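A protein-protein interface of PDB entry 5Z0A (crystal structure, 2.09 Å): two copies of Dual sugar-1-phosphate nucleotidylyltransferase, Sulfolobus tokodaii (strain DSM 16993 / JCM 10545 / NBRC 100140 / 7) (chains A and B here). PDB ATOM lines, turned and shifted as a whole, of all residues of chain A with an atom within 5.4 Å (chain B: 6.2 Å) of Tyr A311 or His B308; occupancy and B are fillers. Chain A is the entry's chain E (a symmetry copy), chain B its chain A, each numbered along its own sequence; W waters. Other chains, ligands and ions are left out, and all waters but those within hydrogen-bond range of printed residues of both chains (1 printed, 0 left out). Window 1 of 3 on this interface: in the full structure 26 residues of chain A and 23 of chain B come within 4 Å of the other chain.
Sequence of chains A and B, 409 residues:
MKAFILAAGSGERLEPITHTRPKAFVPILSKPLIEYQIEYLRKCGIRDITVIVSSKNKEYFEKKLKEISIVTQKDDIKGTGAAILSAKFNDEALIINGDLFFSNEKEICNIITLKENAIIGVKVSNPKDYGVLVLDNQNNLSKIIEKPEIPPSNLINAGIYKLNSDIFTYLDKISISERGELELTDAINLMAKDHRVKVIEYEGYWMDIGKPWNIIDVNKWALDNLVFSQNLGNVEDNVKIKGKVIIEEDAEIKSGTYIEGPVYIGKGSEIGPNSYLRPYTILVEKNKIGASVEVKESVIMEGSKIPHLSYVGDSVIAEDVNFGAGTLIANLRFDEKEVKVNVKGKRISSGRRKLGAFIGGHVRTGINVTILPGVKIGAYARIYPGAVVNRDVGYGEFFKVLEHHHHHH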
ATOM      1  N   ARG A 278     -23.399  -4.482  -5.915  1.00  0.00           N
ATOM      2  CA  ARG A 278     -22.980  -5.768  -5.296  1.00  0.00           C
ATOM      3  C   ARG A 278     -23.701  -6.974  -5.871  1.00  0.00           C
ATOM      4  O   ARG A 278     -24.681  -6.801  -6.587  1.00  0.00           O
ATOM      5  CB  ARG A 278     -23.157  -5.664  -3.808  1.00  0.00           C
ATOM      6  CG  ARG A 278     -21.945  -4.890  -3.245  1.00  0.00           C
ATOM      7  CD  ARG A 278     -22.127  -4.583  -1.775  1.00  0.00           C
ATOM      8  NE  ARG A 278     -22.094  -5.761  -0.946  1.00  0.00           N
ATOM      9  CZ  ARG A 278     -22.601  -5.800   0.288  1.00  0.00           C
ATOM     10  NH1 ARG A 278     -23.229  -4.761   0.823  1.00  0.00           N
ATOM     11  NH2 ARG A 278     -22.570  -6.925   0.980  1.00  0.00           N
ATOM     12  N   GLU A 294     -25.216   2.508  -3.125  1.00  0.00           N
ATOM     13  CA  GLU A 294     -24.820   1.102  -3.039  1.00  0.00           C
ATOM     14  C   GLU A 294     -26.062   0.219  -3.072  1.00  0.00           C
ATOM     15  O   GLU A 294     -27.028   0.499  -2.391  1.00  0.00           O
ATOM     16  CB  GLU A 294     -24.006   0.827  -1.804  1.00  0.00           C
ATOM     17  CG  GLU A 294     -23.625  -0.656  -1.592  1.00  0.00           C
ATOM     18  CD  GLU A 294     -22.808  -0.909  -0.341  1.00  0.00           C
ATOM     19  OE1 GLU A 294     -22.241   0.040   0.230  1.00  0.00           O
ATOM     20  OE2 GLU A 294     -22.814  -2.077   0.095  1.00  0.00           O
ATOM     21  N   VAL A 295     -26.042  -0.778  -3.927  1.00  0.00           N
ATOM     22  CA  VAL A 295     -27.161  -1.743  -4.047  1.00  0.00           C
ATOM     23  C   VAL A 295     -26.591  -3.168  -3.903  1.00  0.00           C
ATOM     24  O   VAL A 295     -25.479  -3.480  -4.419  1.00  0.00           O
ATOM     25  CB  VAL A 295     -27.904  -1.636  -5.386  1.00  0.00           C
ATOM     26  CG1 VAL A 295     -29.078  -2.589  -5.440  1.00  0.00           C
ATOM     27  CG2 VAL A 295     -28.397  -0.253  -5.598  1.00  0.00           C
ATOM     28  N   LYS A 296     -27.307  -3.984  -3.121  1.00  0.00           N
ATOM     29  CA  LYS A 296     -26.968  -5.396  -2.926  1.00  0.00           C
ATOM     30  C   LYS A 296     -28.210  -6.268  -2.835  1.00  0.00           C
ATOM     31  O   LYS A 296     -29.139  -5.940  -2.109  1.00  0.00           O
ATOM     32  CB  LYS A 296     -26.160  -5.541  -1.607  1.00  0.00           C
ATOM     33  CG  LYS A 296     -25.843  -6.944  -1.153  1.00  0.00           C
ATOM     34  CD  LYS A 296     -26.353  -7.145   0.300  1.00  0.00           C
ATOM     35  CE  LYS A 296     -26.197  -8.601   0.727  1.00  0.00           C
ATOM     36  NZ  LYS A 296     -26.765  -8.661   2.084  1.00  0.00           N
ATOM     37  N   LEU A 309     -26.569   9.011  -2.327  1.00  0.00           N
ATOM     38  CA  LEU A 309     -26.265   8.756  -0.912  1.00  0.00           C
ATOM     39  C   LEU A 309     -27.212   7.758  -0.210  1.00  0.00           C
ATOM     40  O   LEU A 309     -27.772   8.062   0.843  1.00  0.00           O
ATOM     41  CB  LEU A 309     -26.230  10.094  -0.158  1.00  0.00           C
ATOM     42  CG  LEU A 309     -25.025  11.042  -0.505  1.00  0.00           C
ATOM     43  CD1 LEU A 309     -25.323  12.540  -0.278  1.00  0.00           C
ATOM     44  CD2 LEU A 309     -23.810  10.642   0.300  1.00  0.00           C
ATOM     45  N   SER A 310     -27.395   6.586  -0.804  1.00  0.00           N
ATOM     46  CA  SER A 310     -28.376   5.592  -0.332  1.00  0.00           C
ATOM     47  C   SER A 310     -27.792   4.198  -0.392  1.00  0.00           C
ATOM     48  O   SER A 310     -26.880   3.915  -1.168  1.00  0.00           O
ATOM     49  CB  SER A 310     -29.690   5.589  -1.163  1.00  0.00           C
ATOM     50  OG  SER A 310     -30.384   6.789  -0.974  1.00  0.00           O
ATOM     51  N   TYR A 311     -28.282   3.357   0.487  1.00  0.00           N
ATOM     52  CA  TYR A 311     -27.939   1.941   0.537  1.00  0.00           C
ATOM     53  C   TYR A 311     -29.230   1.107   0.489  1.00  0.00           C
ATOM     54  O   TYR A 311     -30.140   1.340   1.312  1.00  0.00           O
ATOM     55  CB  TYR A 311     -27.140   1.547   1.776  1.00  0.00           C
ATOM     56  CG  TYR A 311     -26.916  -0.003   1.839  1.00  0.00           C
ATOM     57  CD1 TYR A 311     -26.333  -0.672   0.799  1.00  0.00           C
ATOM     58  CD2 TYR A 311     -27.291  -0.735   2.929  1.00  0.00           C
ATOM     59  CE1 TYR A 311     -26.176  -2.064   0.822  1.00  0.00           C
ATOM     60  CE2 TYR A 311     -27.115  -2.137   2.988  1.00  0.00           C
ATOM     61  CZ  TYR A 311     -26.584  -2.804   1.941  1.00  0.00           C
ATOM     62  OH  TYR A 311     -26.383  -4.199   1.972  1.00  0.00           O
ATOM     63  N   VAL A 312     -29.315   0.237  -0.519  1.00  0.00           N
ATOM     64  CA  VAL A 312     -30.479  -0.646  -0.732  1.00  0.00           C
ATOM     65  C   VAL A 312     -29.957  -2.097  -0.751  1.00  0.00           C
ATOM     66  O   VAL A 312     -29.298  -2.495  -1.688  1.00  0.00           O
ATOM     67  CB  VAL A 312     -31.193  -0.327  -2.065  1.00  0.00           C
ATOM     68  CG1 VAL A 312     -32.373  -1.270  -2.324  1.00  0.00           C
ATOM     69  CG2 VAL A 312     -31.729   1.109  -2.053  1.00  0.00           C
ATOM     70  N   GLY A 313     -30.247  -2.820   0.315  1.00  0.00           N
ATOM     71  CA  GLY A 313     -29.860  -4.185   0.501  1.00  0.00           C
ATOM     72  C   GLY A 313     -31.035  -5.095   0.745  1.00  0.00           C
ATOM     73  O   GLY A 313     -31.938  -4.768   1.503  1.00  0.00           O
ATOM     74  N   ASP A 314     -31.024  -6.224   0.062  1.00  0.00           N
ATOM     75  CA  ASP A 314     -31.982  -7.290   0.336  1.00  0.00           C
ATOM     76  C   ASP A 314     -33.431  -6.832   0.248  1.00  0.00           C
ATOM     77  O   ASP A 314     -34.264  -7.169   1.120  1.00  0.00           O
ATOM     78  CB  ASP A 314     -31.669  -7.919   1.716  1.00  0.00           C
ATOM     79  CG  ASP A 314     -30.295  -8.543   1.792  1.00  0.00           C
ATOM     80  OD1 ASP A 314     -30.083  -9.633   1.243  1.00  0.00           O
ATOM     81  OD2 ASP A 314     -29.382  -7.959   2.438  1.00  0.00           O
ATOM     82  N   THR A 327     -31.905   8.324   1.791  1.00  0.00           N
ATOM     83  CA  THR A 327     -32.810   7.236   2.210  1.00  0.00           C
ATOM     84  C   THR A 327     -31.998   5.974   2.372  1.00  0.00           C
ATOM     85  O   THR A 327     -31.238   5.575   1.484  1.00  0.00           O
ATOM     86  CB  THR A 327     -33.906   6.982   1.123  1.00  0.00           C
ATOM     87  OG1 THR A 327     -34.656   8.212   0.948  1.00  0.00           O
ATOM     88  CG2 THR A 327     -34.825   5.907   1.519  1.00  0.00           C
ATOM     89  N   LEU A 328     -32.182   5.333   3.502  1.00  0.00           N
ATOM     90  CA  LEU A 328     -31.453   4.143   3.883  1.00  0.00           C
ATOM     91  C   LEU A 328     -32.429   3.069   4.295  1.00  0.00           C
ATOM     92  O   LEU A 328     -33.388   3.336   5.042  1.00  0.00           O
ATOM     93  CB  LEU A 328     -30.535   4.396   5.099  1.00  0.00           C
ATOM     94  CG  LEU A 328     -29.485   5.460   4.903  1.00  0.00           C
ATOM     95  CD1 LEU A 328     -28.711   5.743   6.154  1.00  0.00           C
ATOM     96  CD2 LEU A 328     -28.500   5.064   3.804  1.00  0.00           C
ATOM     97  N   ILE A 329     -32.135   1.853   3.877  1.00  0.00           N
ATOM     98  CA  ILE A 329     -32.827   0.646   4.332  1.00  0.00           C
ATOM     99  C   ILE A 329     -31.971  -0.182   5.291  1.00  0.00           C
ATOM    100  O   ILE A 329     -30.878  -0.595   4.948  1.00  0.00           O
ATOM    101  CB  ILE A 329     -33.213  -0.199   3.093  1.00  0.00           C
ATOM    102  CG1 ILE A 329     -34.237   0.594   2.288  1.00  0.00           C
ATOM    103  CG2 ILE A 329     -33.715  -1.545   3.534  1.00  0.00           C
ATOM    104  CD1 ILE A 329     -34.637  -0.028   0.991  1.00  0.00           C
ATOM    105  N   ASN A 331     -31.355  -3.756   6.989  1.00  0.00           N
ATOM    106  CA  ASN A 331     -31.594  -5.134   6.584  1.00  0.00           C
ATOM    107  C   ASN A 331     -31.196  -6.179   7.617  1.00  0.00           C
ATOM    108  O   ASN A 331     -31.164  -7.370   7.286  1.00  0.00           O
ATOM    109  CB  ASN A 331     -30.959  -5.457   5.227  1.00  0.00           C
ATOM    110  CG  ASN A 331     -29.467  -5.304   5.250  1.00  0.00           C
ATOM    111  OD1 ASN A 331     -28.936  -4.633   6.124  1.00  0.00           O
ATOM    112  ND2 ASN A 331     -28.795  -5.894   4.288  1.00  0.00           N
ATOM    113  N   GLY B 290     -16.212   0.362   4.121  1.00  0.00           N
ATOM    114  CA  GLY B 290     -16.952   0.149   2.859  1.00  0.00           C
ATOM    115  C   GLY B 290     -17.089   1.372   2.030  1.00  0.00           C
ATOM    116  O   GLY B 290     -16.365   2.393   2.216  1.00  0.00           O
ATOM    117  N   ALA B 291     -18.021   1.316   1.087  1.00  0.00           N
ATOM    118  CA  ALA B 291     -18.212   2.410   0.094  1.00  0.00           C
ATOM    119  C   ALA B 291     -18.758   3.644   0.751  1.00  0.00           C
ATOM    120  O   ALA B 291     -19.703   3.557   1.554  1.00  0.00           O
ATOM    121  CB  ALA B 291     -19.131   1.979  -1.018  1.00  0.00           C
ATOM    122  N   SER B 292     -18.223   4.780   0.338  1.00  0.00           N
ATOM    123  CA  SER B 292     -18.560   6.120   0.875  1.00  0.00           C
ATOM    124  C   SER B 292     -18.367   6.214   2.365  1.00  0.00           C
ATOM    125  O   SER B 292     -19.185   6.777   3.077  1.00  0.00           O
ATOM    126  CB  SER B 292     -20.025   6.499   0.494  1.00  0.00           C
ATOM    127  OG  SER B 292     -20.265   6.399  -0.873  1.00  0.00           O
ATOM    128  N   VAL B 293     -17.328   5.532   2.854  1.00  0.00           N
ATOM    129  CA  VAL B 293     -16.916   5.591   4.234  1.00  0.00           C
ATOM    130  C   VAL B 293     -15.617   6.335   4.286  1.00  0.00           C
ATOM    131  O   VAL B 293     -14.671   6.026   3.537  1.00  0.00           O
ATOM    132  CB  VAL B 293     -16.798   4.208   4.916  1.00  0.00           C
ATOM    133  CG1 VAL B 293     -16.284   4.343   6.329  1.00  0.00           C
ATOM    134  CG2 VAL B 293     -18.165   3.529   4.948  1.00  0.00           C
ATOM    135  N   ILE B 306     -17.400  -0.688   9.544  1.00  0.00           N
ATOM    136  CA  ILE B 306     -18.070   0.575   9.175  1.00  0.00           C
ATOM    137  C   ILE B 306     -18.431   0.474   7.709  1.00  0.00           C
ATOM    138  O   ILE B 306     -17.609   0.881   6.841  1.00  0.00           O
ATOM    139  CB  ILE B 306     -17.186   1.791   9.390  1.00  0.00           C
ATOM    140  CG1 ILE B 306     -16.346   1.758  10.695  1.00  0.00           C
ATOM    141  CG2 ILE B 306     -18.053   3.042   9.287  1.00  0.00           C
ATOM    142  CD1 ILE B 306     -17.128   1.884  11.943  1.00  0.00           C
ATOM    143  N   PRO B 307     -19.541  -0.231   7.380  1.00  0.00           N
ATOM    144  CA  PRO B 307     -19.676  -0.721   5.980  1.00  0.00           C
ATOM    145  C   PRO B 307     -20.229   0.274   4.964  1.00  0.00           C
ATOM    146  O   PRO B 307     -19.988   0.102   3.782  1.00  0.00           O
ATOM    147  CB  PRO B 307     -20.608  -1.961   6.124  1.00  0.00           C
ATOM    148  CG  PRO B 307     -21.361  -1.683   7.388  1.00  0.00           C
ATOM    149  CD  PRO B 307     -20.407  -0.954   8.289  1.00  0.00           C
ATOM    150  N   HIS B 308     -20.941   1.344   5.384  1.00  0.00           N
ATOM    151  CA  HIS B 308     -21.611   2.234   4.383  1.00  0.00           C
ATOM    152  C   HIS B 308     -21.846   3.616   4.833  1.00  0.00           C
ATOM    153  O   HIS B 308     -22.437   3.795   5.880  1.00  0.00           O
ATOM    154  CB  HIS B 308     -23.051   1.732   4.015  1.00  0.00           C
ATOM    155  CG  HIS B 308     -23.224   0.246   3.975  1.00  0.00           C
ATOM    156  ND1 HIS B 308     -22.963  -0.510   2.852  1.00  0.00           N
ATOM    157  CD2 HIS B 308     -23.691  -0.614   4.915  1.00  0.00           C
ATOM    158  CE1 HIS B 308     -23.235  -1.781   3.117  1.00  0.00           C
ATOM    159  NE2 HIS B 308     -23.724  -1.858   4.348  1.00  0.00           N
ATOM    160  N   LEU B 309     -21.479   4.622   3.990  1.00  0.00           N
ATOM    161  CA  LEU B 309     -22.010   5.951   4.113  1.00  0.00           C
ATOM    162  C   LEU B 309     -21.803   6.594   5.494  1.00  0.00           C
ATOM    163  O   LEU B 309     -22.743   7.054   6.115  1.00  0.00           O
ATOM    164  CB  LEU B 309     -23.512   5.953   3.732  1.00  0.00           C
ATOM    165  CG  LEU B 309     -23.837   5.758   2.232  1.00  0.00           C
ATOM    166  CD1 LEU B 309     -25.214   5.137   1.928  1.00  0.00           C
ATOM    167  CD2 LEU B 309     -23.692   7.095   1.500  1.00  0.00           C
ATOM    168  N   SER B 310     -20.575   6.538   5.997  1.00  0.00           N
ATOM    169  CA  SER B 310     -20.272   6.951   7.369  1.00  0.00           C
ATOM    170  C   SER B 310     -19.009   7.790   7.366  1.00  0.00           C
ATOM    171  O   SER B 310     -18.138   7.610   6.527  1.00  0.00           O
ATOM    172  CB  SER B 310     -20.096   5.772   8.333  1.00  0.00           C
ATOM    173  OG  SER B 310     -21.310   5.099   8.543  1.00  0.00           O
ATOM    174  N   PHE B 323     -21.313  -0.403  12.750  1.00  0.00           N
ATOM    175  CA  PHE B 323     -22.003   0.821  12.426  1.00  0.00           C
ATOM    176  C   PHE B 323     -23.010   0.603  11.282  1.00  0.00           C
ATOM    177  O   PHE B 323     -22.624   0.285  10.191  1.00  0.00           O
ATOM    178  CB  PHE B 323     -21.062   1.912  11.999  1.00  0.00           C
ATOM    179  CG  PHE B 323     -20.487   2.729  13.140  1.00  0.00           C
ATOM    180  CD1 PHE B 323     -20.497   2.277  14.455  1.00  0.00           C
ATOM    181  CD2 PHE B 323     -19.971   3.989  12.875  1.00  0.00           C
ATOM    182  CE1 PHE B 323     -19.962   3.075  15.482  1.00  0.00           C
ATOM    183  CE2 PHE B 323     -19.433   4.782  13.900  1.00  0.00           C
ATOM    184  CZ  PHE B 323     -19.432   4.334  15.194  1.00  0.00           C
ATOM    185  N   GLY B 324     -24.288   0.748  11.587  1.00  0.00           N
ATOM    186  CA  GLY B 324     -25.296   0.713  10.553  1.00  0.00           C
ATOM    187  C   GLY B 324     -24.968   1.824   9.530  1.00  0.00           C
ATOM    188  O   GLY B 324     -24.333   2.875   9.856  1.00  0.00           O
ATOM    189  N   ALA B 325     -25.367   1.591   8.289  1.00  0.00           N
ATOM    190  CA  ALA B 325     -25.283   2.627   7.248  1.00  0.00           C
ATOM    191  C   ALA B 325     -25.726   3.991   7.737  1.00  0.00           C
ATOM    192  O   ALA B 325     -26.787   4.142   8.378  1.00  0.00           O
ATOM    193  CB  ALA B 325     -26.140   2.216   6.039  1.00  0.00           C
ATOM    194  N   GLY B 326     -24.957   4.998   7.354  1.00  0.00           N
ATOM    195  CA  GLY B 326     -25.285   6.421   7.669  1.00  0.00           C
ATOM    196  C   GLY B 326     -25.049   6.830   9.072  1.00  0.00           C
ATOM    197  O   GLY B 326     -25.575   7.844   9.475  1.00  0.00           O
ATOM    198  N   THR B 327     -24.364   6.028   9.881  1.00  0.00           N
ATOM    199  CA  THR B 327     -23.957   6.451  11.214  1.00  0.00           C
ATOM    200  C   THR B 327     -22.851   7.504  11.055  1.00  0.00           C
ATOM    201  O   THR B 327     -21.866   7.264  10.352  1.00  0.00           O
ATOM    202  CB  THR B 327     -23.413   5.244  12.057  1.00  0.00           C
ATOM    203  OG1 THR B 327     -24.478   4.283  12.200  1.00  0.00           O
ATOM    204  CG2 THR B 327     -22.982   5.663  13.414  1.00  0.00           C
HETATM  205  O   HOH W   1     -22.168   2.553   0.991  1.00  0.00           O
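Of the 14 printed residues of chain B, 5 touch a printed residue of chain A. Hydrophobic or aromatic side chains of chain B within 4 Å of the printed part of chain A: Ala B291, His B308 and Leu B309. Of the 14 printed residues of chain A, 6 touch a printed residue of chain B. Hydrophobic or aromatic side chains of chain A within 4 Å of the printed part of chain B: Leu A309, Tyr A311 and Leu A328.
ND1 of His B308 sits at hydrogen-bond distance from OE1 of Glu A294 (2.8 Å).
Leu A309 touches its own counterpart, Leu B309. Ser A310 touches Leu B309, but with the chains exchanged Leu A309 does not touch Ser B310 (7.7 Å). Positions printed for both chains: 309, 310 and 327. Of the 10 pairs that touch across the chains among the printed residues, 1 has its exchanged pair printed and touching as well.
Among the printed residues, merely in contact across the chains: Leu A328 with Ala B325 (3.3 Å), Ser A310 with Leu B309 (3.6 Å), Tyr A311 with His B308 (3.7 Å), Leu A309 with Leu B309 (3.7 Å), Arg A278 with His B308 (3.8 Å), Leu A328 with Leu B309 (3.8 Å), Leu A328 with Gly B326 (3.8 Å), Tyr A311 with Leu B309 (3.8 Å) and Glu A294 with Ala B291 (3.9 Å).
Printed residues of chain B within 4 Å of Arg A278: His B308 (3.8 Å). Tyr A311 touches just these residues of chain B: His B308 (3.7 Å) and Leu B309 (3.8 Å). Of the printed residues of chain B, Leu A328 touches Leu B309, Ala B325 and Gly B326. His B308 touches three residues of chain A. The nearest printed residue of chain A that does not touch His B308 is Asn A331 (6.2 Å).
O of His B308 is in hydrogen-bond range of OG of Ser B310 (3.2 Å). The backbone carbonyl oxygen (O) of His B308 is in hydrogen-bond range of the backbone NH (N) of Gly B326, 3.2 Å away. The guanidinium group of Arg A278 is in salt-bridge range of the side-chain carboxylate of Glu A294 (2.8 Å). The guanidinium group (NH1) of Arg A278 lies within hydrogen-bond range of the side-chain hydroxyl (OH) of Tyr A311, 3.4 Å away. The backbone carbonyl oxygen of Ser A310 lies within hydrogen-bond range of the backbone NH of Glu A294, 2.9 Å away. N of Val A312 lies within hydrogen-bond range of O of Glu A294, 3.0 Å away.
Water W1 lies within hydrogen-bond range of OE1 of Glu A294 (2.6 Å) and O of Ala B291 (2.7 Å).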
